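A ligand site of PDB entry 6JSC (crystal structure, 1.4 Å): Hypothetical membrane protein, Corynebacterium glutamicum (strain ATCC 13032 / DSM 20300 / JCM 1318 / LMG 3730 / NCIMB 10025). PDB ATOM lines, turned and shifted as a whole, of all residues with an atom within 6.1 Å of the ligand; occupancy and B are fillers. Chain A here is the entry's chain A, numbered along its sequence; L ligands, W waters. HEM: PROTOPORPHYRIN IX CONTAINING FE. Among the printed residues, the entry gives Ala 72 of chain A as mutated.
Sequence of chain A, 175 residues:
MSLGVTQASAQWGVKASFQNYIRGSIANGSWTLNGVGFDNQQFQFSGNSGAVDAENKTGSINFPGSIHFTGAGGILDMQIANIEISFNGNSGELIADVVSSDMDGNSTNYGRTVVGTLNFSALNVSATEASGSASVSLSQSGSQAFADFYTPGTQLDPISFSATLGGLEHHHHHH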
ATOM      1  N   LYS A  15      -3.552  14.709 -20.700  1.00  0.00           N
ATOM      2  CA  LYS A  15      -3.392  15.535 -21.898  1.00  0.00           C
ATOM      3  C   LYS A  15      -2.024  16.206 -21.832  1.00  0.00           C
ATOM      4  O   LYS A  15      -1.684  16.842 -20.825  1.00  0.00           O
ATOM      5  CB  LYS A  15      -4.502  16.595 -22.033  1.00  0.00           C
ATOM      6  CG  LYS A  15      -4.604  17.203 -23.425  1.00  0.00           C
ATOM      7  CD  LYS A  15      -5.677  18.297 -23.473  1.00  0.00           C
ATOM      8  CE  LYS A  15      -5.987  18.797 -24.884  1.00  0.00           C
ATOM      9  NZ  LYS A  15      -4.793  19.322 -25.605  1.00  0.00           N
ATOM     10  N   ALA A  16      -1.240  16.072 -22.900  1.00  0.00           N
ATOM     11  CA  ALA A  16       0.112  16.611 -22.888  1.00  0.00           C
ATOM     12  C   ALA A  16       0.115  18.118 -22.597  1.00  0.00           C
ATOM     13  O   ALA A  16       0.925  18.602 -21.802  1.00  0.00           O
ATOM     14  CB  ALA A  16       0.799  16.314 -24.226  1.00  0.00           C
ATOM     15  N   SER A  17      -0.791  18.866 -23.237  1.00  0.00           N
ATOM     16  CA  SER A  17      -0.812  20.310 -22.998  1.00  0.00           C
ATOM     17  C   SER A  17      -1.240  20.642 -21.578  1.00  0.00           C
ATOM     18  O   SER A  17      -0.848  21.691 -21.045  1.00  0.00           O
ATOM     19  CB  SER A  17      -1.706  21.011 -24.032  1.00  0.00           C
ATOM     20  OG  SER A  17      -3.059  20.637 -23.875  1.00  0.00           O
ATOM     21  N   PHE A  18      -2.018  19.771 -20.936  1.00  0.00           N
ATOM     22  CA  PHE A  18      -2.360  19.986 -19.525  1.00  0.00           C
ATOM     23  C   PHE A  18      -1.152  19.775 -18.617  1.00  0.00           C
ATOM     24  O   PHE A  18      -0.936  20.549 -17.690  1.00  0.00           O
ATOM     25  CB  PHE A  18      -3.535  19.088 -19.101  1.00  0.00           C
ATOM     26  CG  PHE A  18      -4.067  19.401 -17.715  1.00  0.00           C
ATOM     27  CD1 PHE A  18      -4.659  20.629 -17.452  1.00  0.00           C
ATOM     28  CD2 PHE A  18      -3.961  18.472 -16.688  1.00  0.00           C
ATOM     29  CE1 PHE A  18      -5.148  20.924 -16.185  1.00  0.00           C
ATOM     30  CE2 PHE A  18      -4.463  18.761 -15.424  1.00  0.00           C
ATOM     31  CZ  PHE A  18      -5.055  19.992 -15.170  1.00  0.00           C
ATOM     32  N   TYR A  21       0.880  22.867 -19.002  1.00  0.00           N
ATOM     33  CA  TYR A  21       0.242  23.979 -18.295  1.00  0.00           C
ATOM     34  C   TYR A  21       0.435  23.866 -16.780  1.00  0.00           C
ATOM     35  O   TYR A  21       0.808  24.845 -16.123  1.00  0.00           O
ATOM     36  CB  TYR A  21      -1.242  24.045 -18.692  1.00  0.00           C
ATOM     37  CG  TYR A  21      -2.092  24.825 -17.707  1.00  0.00           C
ATOM     38  CD1 TYR A  21      -2.033  26.214 -17.680  1.00  0.00           C
ATOM     39  CD2 TYR A  21      -2.931  24.175 -16.800  1.00  0.00           C
ATOM     40  CE1 TYR A  21      -2.791  26.928 -16.763  1.00  0.00           C
ATOM     41  CE2 TYR A  21      -3.688  24.895 -15.901  1.00  0.00           C
ATOM     42  CZ  TYR A  21      -3.616  26.262 -15.891  1.00  0.00           C
ATOM     43  OH  TYR A  21      -4.344  27.005 -14.993  1.00  0.00           O
ATOM     44  N   ILE A  26       1.920  29.765 -15.542  1.00  0.00           N
ATOM     45  CA  ILE A  26       0.601  30.301 -15.239  1.00  0.00           C
ATOM     46  C   ILE A  26       0.034  29.552 -14.038  1.00  0.00           C
ATOM     47  O   ILE A  26      -0.207  30.154 -12.979  1.00  0.00           O
ATOM     48  CB  ILE A  26      -0.337  30.223 -16.462  1.00  0.00           C
ATOM     49  CG1 ILE A  26       0.258  31.016 -17.626  1.00  0.00           C
ATOM     50  CG2 ILE A  26      -1.732  30.745 -16.106  1.00  0.00           C
ATOM     51  CD1 ILE A  26      -0.515  30.873 -18.930  1.00  0.00           C
ATOM     52  N   ALA A  27      -0.151  28.239 -14.186  1.00  0.00           N
ATOM     53  CA  ALA A  27      -0.619  27.445 -13.055  1.00  0.00           C
ATOM     54  C   ALA A  27       0.407  27.392 -11.931  1.00  0.00           C
ATOM     55  O   ALA A  27       0.035  27.331 -10.758  1.00  0.00           O
ATOM     56  CB  ALA A  27      -0.974  26.036 -13.489  1.00  0.00           C
ATOM     57  N   ALA A  72      -2.428  27.287  -9.306  1.00  0.00           N
ATOM     58  CA  ALA A  72      -3.114  28.554  -9.059  1.00  0.00           C
ATOM     59  C   ALA A  72      -3.241  28.832  -7.569  1.00  0.00           C
ATOM     60  O   ALA A  72      -4.293  29.230  -7.080  1.00  0.00           O
ATOM     61  CB  ALA A  72      -4.469  28.626  -9.770  1.00  0.00           C
ATOM     62  N   ILE A  75      -6.144  27.037  -5.868  1.00  0.00           N
ATOM     63  CA  ILE A  75      -7.470  27.121  -6.479  1.00  0.00           C
ATOM     64  C   ILE A  75      -7.710  25.940  -7.400  1.00  0.00           C
ATOM     65  O   ILE A  75      -8.818  25.376  -7.433  1.00  0.00           O
ATOM     66  CB  ILE A  75      -7.629  28.477  -7.195  1.00  0.00           C
ATOM     67  CG1 ILE A  75      -7.631  29.622  -6.177  1.00  0.00           C
ATOM     68  CG2 ILE A  75      -8.895  28.481  -8.026  1.00  0.00           C
ATOM     69  CD1 ILE A  75      -7.579  30.995  -6.808  1.00  0.00           C
ATOM     70  N   LEU A  76      -6.704  25.563  -8.191  1.00  0.00           N
ATOM     71  CA  LEU A  76      -6.791  24.353  -8.995  1.00  0.00           C
ATOM     72  C   LEU A  76      -6.462  23.164  -8.097  1.00  0.00           C
ATOM     73  O   LEU A  76      -5.396  23.123  -7.471  1.00  0.00           O
ATOM     74  CB  LEU A  76      -5.853  24.431 -10.193  1.00  0.00           C
ATOM     75  CG  LEU A  76      -6.006  23.399 -11.313  1.00  0.00           C
ATOM     76  CD1 LEU A  76      -5.363  23.887 -12.614  1.00  0.00           C
ATOM     77  CD2 LEU A  76      -5.411  22.048 -10.899  1.00  0.00           C
ATOM     78  N   ASP A  77      -7.375  22.202  -8.021  1.00  0.00           N
ATOM     79  CA  ASP A  77      -7.210  21.063  -7.130  1.00  0.00           C
ATOM     80  C   ASP A  77      -8.087  19.967  -7.736  1.00  0.00           C
ATOM     81  O   ASP A  77      -9.305  19.979  -7.540  1.00  0.00           O
ATOM     82  CB  ASP A  77      -7.649  21.425  -5.721  1.00  0.00           C
ATOM     83  CG  ASP A  77      -7.291  20.371  -4.694  1.00  0.00           C
ATOM     84  OD1 ASP A  77      -7.378  19.174  -5.020  1.00  0.00           O
ATOM     85  OD2 ASP A  77      -6.928  20.752  -3.556  1.00  0.00           O
ATOM     86  N   MET A  78      -7.463  19.063  -8.482  1.00  0.00           N
ATOM     87  CA  MET A  78      -8.176  18.060  -9.267  1.00  0.00           C
ATOM     88  C   MET A  78      -7.595  16.683  -8.957  1.00  0.00           C
ATOM     89  O   MET A  78      -6.383  16.466  -9.103  1.00  0.00           O
ATOM     90  CB  MET A  78      -8.036  18.370 -10.757  1.00  0.00           C
ATOM     91  CG  MET A  78      -8.805  17.402 -11.651  1.00  0.00           C
ATOM     92  SD  MET A  78      -8.498  17.732 -13.406  1.00  0.00           S
ATOM     93  CE  MET A  78      -9.954  17.000 -14.171  1.00  0.00           C
ATOM     94  N   SER A 100     -12.939  17.999  -8.290  1.00  0.00           N
ATOM     95  CA  SER A 100     -12.198  19.125  -8.853  1.00  0.00           C
ATOM     96  C   SER A 100     -12.767  20.462  -8.385  1.00  0.00           C
ATOM     97  O   SER A 100     -13.980  20.658  -8.372  1.00  0.00           O
ATOM     98  CB  SER A 100     -12.214  19.080 -10.384  1.00  0.00           C
ATOM     99  OG  SER A 100     -11.268  20.000 -10.924  1.00  0.00           O
ATOM    100  N   SER A 101     -11.873  21.390  -8.053  1.00  0.00           N
ATOM    101  CA  SER A 101     -12.287  22.718  -7.618  1.00  0.00           C
ATOM    102  C   SER A 101     -12.553  23.628  -8.810  1.00  0.00           C
ATOM    103  O   SER A 101     -11.911  23.536  -9.854  1.00  0.00           O
ATOM    104  CB  SER A 101     -11.233  23.346  -6.717  1.00  0.00           C
ATOM    105  OG  SER A 101     -11.144  22.654  -5.489  1.00  0.00           O
ATOM    106  N   ASP A 102     -13.529  24.520  -8.631  1.00  0.00           N
ATOM    107  CA  ASP A 102     -13.865  25.516  -9.644  1.00  0.00           C
ATOM    108  C   ASP A 102     -12.953  26.731  -9.513  1.00  0.00           C
ATOM    109  O   ASP A 102     -12.068  26.784  -8.650  1.00  0.00           O
ATOM    110  CB  ASP A 102     -15.358  25.849  -9.608  1.00  0.00           C
ATOM    111  CG  ASP A 102     -15.801  26.517  -8.303  1.00  0.00           C
ATOM    112  OD1 ASP A 102     -14.963  27.092  -7.572  1.00  0.00           O
ATOM    113  OD2 ASP A 102     -17.018  26.492  -8.003  1.00  0.00           O
ATOM    114  N   MET A 103     -13.172  27.741 -10.365  1.00  0.00           N
ATOM    115  CA  MET A 103     -12.260  28.878 -10.364  1.00  0.00           C
ATOM    116  C   MET A 103     -12.434  29.779  -9.143  1.00  0.00           C
ATOM    117  O   MET A 103     -11.605  30.685  -8.938  1.00  0.00           O
ATOM    118  CB  MET A 103     -12.294  29.647 -11.711  1.00  0.00           C
ATOM    119  CG  MET A 103     -11.441  29.019 -12.878  1.00  0.00           C
ATOM    120  SD  MET A 103     -11.301  30.172 -14.257  1.00  0.00           S
ATOM    121  CE  MET A 103     -10.508  31.553 -13.450  1.00  0.00           C
ATOM    122  N   ALA A 145     -15.153  19.515 -14.888  1.00  0.00           N
ATOM    123  CA  ALA A 145     -14.058  19.313 -13.954  1.00  0.00           C
ATOM    124  C   ALA A 145     -12.814  20.101 -14.356  1.00  0.00           C
ATOM    125  O   ALA A 145     -12.043  20.526 -13.477  1.00  0.00           O
ATOM    126  CB  ALA A 145     -13.736  17.816 -13.839  1.00  0.00           C
ATOM    127  N   PHE A 146     -12.594  20.317 -15.659  1.00  0.00           N
ATOM    128  CA  PHE A 146     -11.508  21.146 -16.144  1.00  0.00           C
ATOM    129  C   PHE A 146     -11.884  22.634 -16.213  1.00  0.00           C
ATOM    130  O   PHE A 146     -11.279  23.390 -16.989  1.00  0.00           O
ATOM    131  CB  PHE A 146     -11.000  20.642 -17.508  1.00  0.00           C
ATOM    132  CG  PHE A 146     -10.090  19.441 -17.433  1.00  0.00           C
ATOM    133  CD1 PHE A 146      -8.781  19.566 -16.988  1.00  0.00           C
ATOM    134  CD2 PHE A 146     -10.515  18.196 -17.883  1.00  0.00           C
ATOM    135  CE1 PHE A 146      -7.938  18.482 -16.955  1.00  0.00           C
ATOM    136  CE2 PHE A 146      -9.675  17.106 -17.863  1.00  0.00           C
ATOM    137  CZ  PHE A 146      -8.380  17.250 -17.392  1.00  0.00           C
ATOM    138  N   ALA A 147     -12.885  23.060 -15.437  1.00  0.00           N
ATOM    139  CA  ALA A 147     -13.270  24.472 -15.310  1.00  0.00           C
ATOM    140  C   ALA A 147     -13.649  25.103 -16.642  1.00  0.00           C
ATOM    141  O   ALA A 147     -13.469  26.314 -16.842  1.00  0.00           O
ATOM    142  CB  ALA A 147     -12.206  25.300 -14.576  1.00  0.00           C
ATOM    143  N   PHE A 149     -12.274  24.983 -19.460  1.00  0.00           N
ATOM    144  CA  PHE A 149     -11.195  25.376 -20.358  1.00  0.00           C
ATOM    145  C   PHE A 149     -11.129  24.498 -21.601  1.00  0.00           C
ATOM    146  O   PHE A 149     -10.635  24.959 -22.638  1.00  0.00           O
ATOM    147  CB  PHE A 149      -9.866  25.376 -19.605  1.00  0.00           C
ATOM    148  CG  PHE A 149      -9.635  26.600 -18.765  1.00  0.00           C
ATOM    149  CD1 PHE A 149      -9.982  26.626 -17.415  1.00  0.00           C
ATOM    150  CD2 PHE A 149      -9.087  27.749 -19.325  1.00  0.00           C
ATOM    151  CE1 PHE A 149      -9.774  27.760 -16.647  1.00  0.00           C
ATOM    152  CE2 PHE A 149      -8.891  28.881 -18.570  1.00  0.00           C
ATOM    153  CZ  PHE A 149      -9.222  28.890 -17.224  1.00  0.00           C
ATOM    154  N   TYR A 150     -11.609  23.259 -21.528  1.00  0.00           N
ATOM    155  CA  TYR A 150     -11.812  22.395 -22.693  1.00  0.00           C
ATOM    156  C   TYR A 150     -13.306  22.198 -22.901  1.00  0.00           C
ATOM    157  O   TYR A 150     -14.049  21.973 -21.934  1.00  0.00           O
ATOM    158  CB  TYR A 150     -11.220  20.993 -22.454  1.00  0.00           C
ATOM    159  CG  TYR A 150      -9.760  20.919 -22.072  1.00  0.00           C
ATOM    160  CD1 TYR A 150      -8.796  21.661 -22.762  1.00  0.00           C
ATOM    161  CD2 TYR A 150      -9.345  20.116 -21.023  1.00  0.00           C
ATOM    162  CE1 TYR A 150      -7.456  21.581 -22.402  1.00  0.00           C
ATOM    163  CE2 TYR A 150      -8.008  20.027 -20.666  1.00  0.00           C
ATOM    164  CZ  TYR A 150      -7.067  20.764 -21.349  1.00  0.00           C
ATOM    165  OH  TYR A 150      -5.747  20.687 -20.979  1.00  0.00           O
HETATM  166  CHA HEM L   1      -5.406  27.276 -18.997  1.00  0.00           C
HETATM  167  CHB HEM L   1      -5.870  30.972 -15.863  1.00  0.00           C
HETATM  168  CHC HEM L   1      -7.828  27.930 -12.636  1.00  0.00           C
HETATM  169  CHD HEM L   1      -7.770  24.364 -15.917  1.00  0.00           C
HETATM  170  C1A HEM L   1      -5.374  28.537 -18.445  1.00  0.00           C
HETATM  171  C2A HEM L   1      -4.901  29.724 -19.103  1.00  0.00           C
HETATM  172  C3A HEM L   1      -5.025  30.744 -18.240  1.00  0.00           C
HETATM  173  C4A HEM L   1      -5.592  30.238 -17.002  1.00  0.00           C
HETATM  174  CMA HEM L   1      -4.628  32.224 -18.506  1.00  0.00           C
HETATM  175  CAA HEM L   1      -4.343  29.769 -20.552  1.00  0.00           C
HETATM  176  CBA HEM L   1      -5.338  30.385 -21.525  1.00  0.00           C
HETATM  177  CGA HEM L   1      -6.363  29.368 -21.980  1.00  0.00           C
HETATM  178  O1A HEM L   1      -7.568  29.711 -21.983  1.00  0.00           O
HETATM  179  O2A HEM L   1      -5.966  28.227 -22.324  1.00  0.00           O
HETATM  180  C1B HEM L   1      -6.452  30.488 -14.704  1.00  0.00           C
HETATM  181  C2B HEM L   1      -6.805  31.244 -13.521  1.00  0.00           C
HETATM  182  C3B HEM L   1      -7.354  30.396 -12.634  1.00  0.00           C
HETATM  183  C4B HEM L   1      -7.344  29.080 -13.232  1.00  0.00           C
HETATM  184  CMB HEM L   1      -6.597  32.776 -13.353  1.00  0.00           C
HETATM  185  CAB HEM L   1      -7.913  30.626 -11.203  1.00  0.00           C
HETATM  186  CBB HEM L   1      -7.755  31.744 -10.497  1.00  0.00           C
HETATM  187  C1C HEM L   1      -8.045  26.726 -13.258  1.00  0.00           C
HETATM  188  C2C HEM L   1      -8.770  25.615 -12.688  1.00  0.00           C
HETATM  189  C3C HEM L   1      -8.744  24.616 -13.574  1.00  0.00           C
HETATM  190  C4C HEM L   1      -8.015  25.066 -14.754  1.00  0.00           C
HETATM  191  CMC HEM L   1      -9.444  25.607 -11.290  1.00  0.00           C
HETATM  192  CAC HEM L   1      -9.397  23.234 -13.391  1.00  0.00           C
HETATM  193  CBC HEM L   1      -8.777  22.133 -13.822  1.00  0.00           C
HETATM  194  C1D HEM L   1      -7.157  24.840 -17.055  1.00  0.00           C
HETATM  195  C2D HEM L   1      -6.978  24.137 -18.308  1.00  0.00           C
HETATM  196  C3D HEM L   1      -6.329  24.937 -19.161  1.00  0.00           C
HETATM  197  C4D HEM L   1      -6.055  26.176 -18.471  1.00  0.00           C
HETATM  198  CMD HEM L   1      -7.494  22.707 -18.582  1.00  0.00           C
HETATM  199  CAD HEM L   1      -5.905  24.593 -20.607  1.00  0.00           C
HETATM  200  CBD HEM L   1      -4.450  24.113 -20.566  1.00  0.00           C
HETATM  201  CGD HEM L   1      -3.978  23.593 -21.906  1.00  0.00           C
HETATM  202  O1D HEM L   1      -4.143  22.380 -22.169  1.00  0.00           O
HETATM  203  O2D HEM L   1      -3.433  24.389 -22.705  1.00  0.00           O
HETATM  204  NA  HEM L   1      -5.783  28.878 -17.167  1.00  0.00           N
HETATM  205  NB  HEM L   1      -6.788  29.163 -14.500  1.00  0.00           N
HETATM  206  NC  HEM L   1      -7.590  26.362 -14.518  1.00  0.00           N
HETATM  207  ND  HEM L   1      -6.571  26.085 -17.192  1.00  0.00           N
HETATM  208 FE   HEM L   1      -6.279  27.510 -15.673  1.00  0.00          FE
HETATM  209  O   HOH W   1      -3.814  28.661 -13.193  1.00  0.00           O
HETATM  210  O   HOH W   2      -8.794  32.040 -21.080  1.00  0.00           O
HETATM  211  O   HOH W   3       0.017  24.016 -22.394  1.00  0.00           O
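Merely in contact with the ligand: Phe 18 (3.6 Å), Ile 26 (3.9 Å), Ile 75 (3.8 Å), Leu 76 (3.6 Å), Ser 101 (3.5 Å), Asp 102 (3.9 Å), Met 103 (3.5 Å), Ala 145 (3.7 Å), Phe 146 (3.7 Å), Ala 147 (3.7 Å) and Phe 149 (3.4 Å). Of the 21 residues printed, 14 come within 4 Å of the ligand. The nearest printed residue that does not touch the ligand is Ala 72 (4.2 Å).
Water W3 lies within hydrogen-bond range of O of Ser 17 (2.8 Å) and O2D of the ligand (3.5 Å).
FE of the ligand is bound by OH of Tyr 21. OH of Tyr 150 sits at hydrogen-bond distance from O1D of the ligand (2.6 Å). The side-chain hydroxyl (OG) of Ser 17 lies within hydrogen-bond range of an oxygen (O1D) of the ligand, 2.7 Å away.
OG of Ser 17 sits at hydrogen-bond distance from NZ of Lys 15, at 2.8 Å. The backbone carbonyl oxygen of Asp 77 lies within hydrogen-bond range of the backbone NH of Ser 101 (3.0 Å). The backbone carbonyl oxygen (O) of Ala 145 lies within hydrogen-bond range of the side-chain hydroxyl (OG) of Ser 100, 2.7 Å away.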
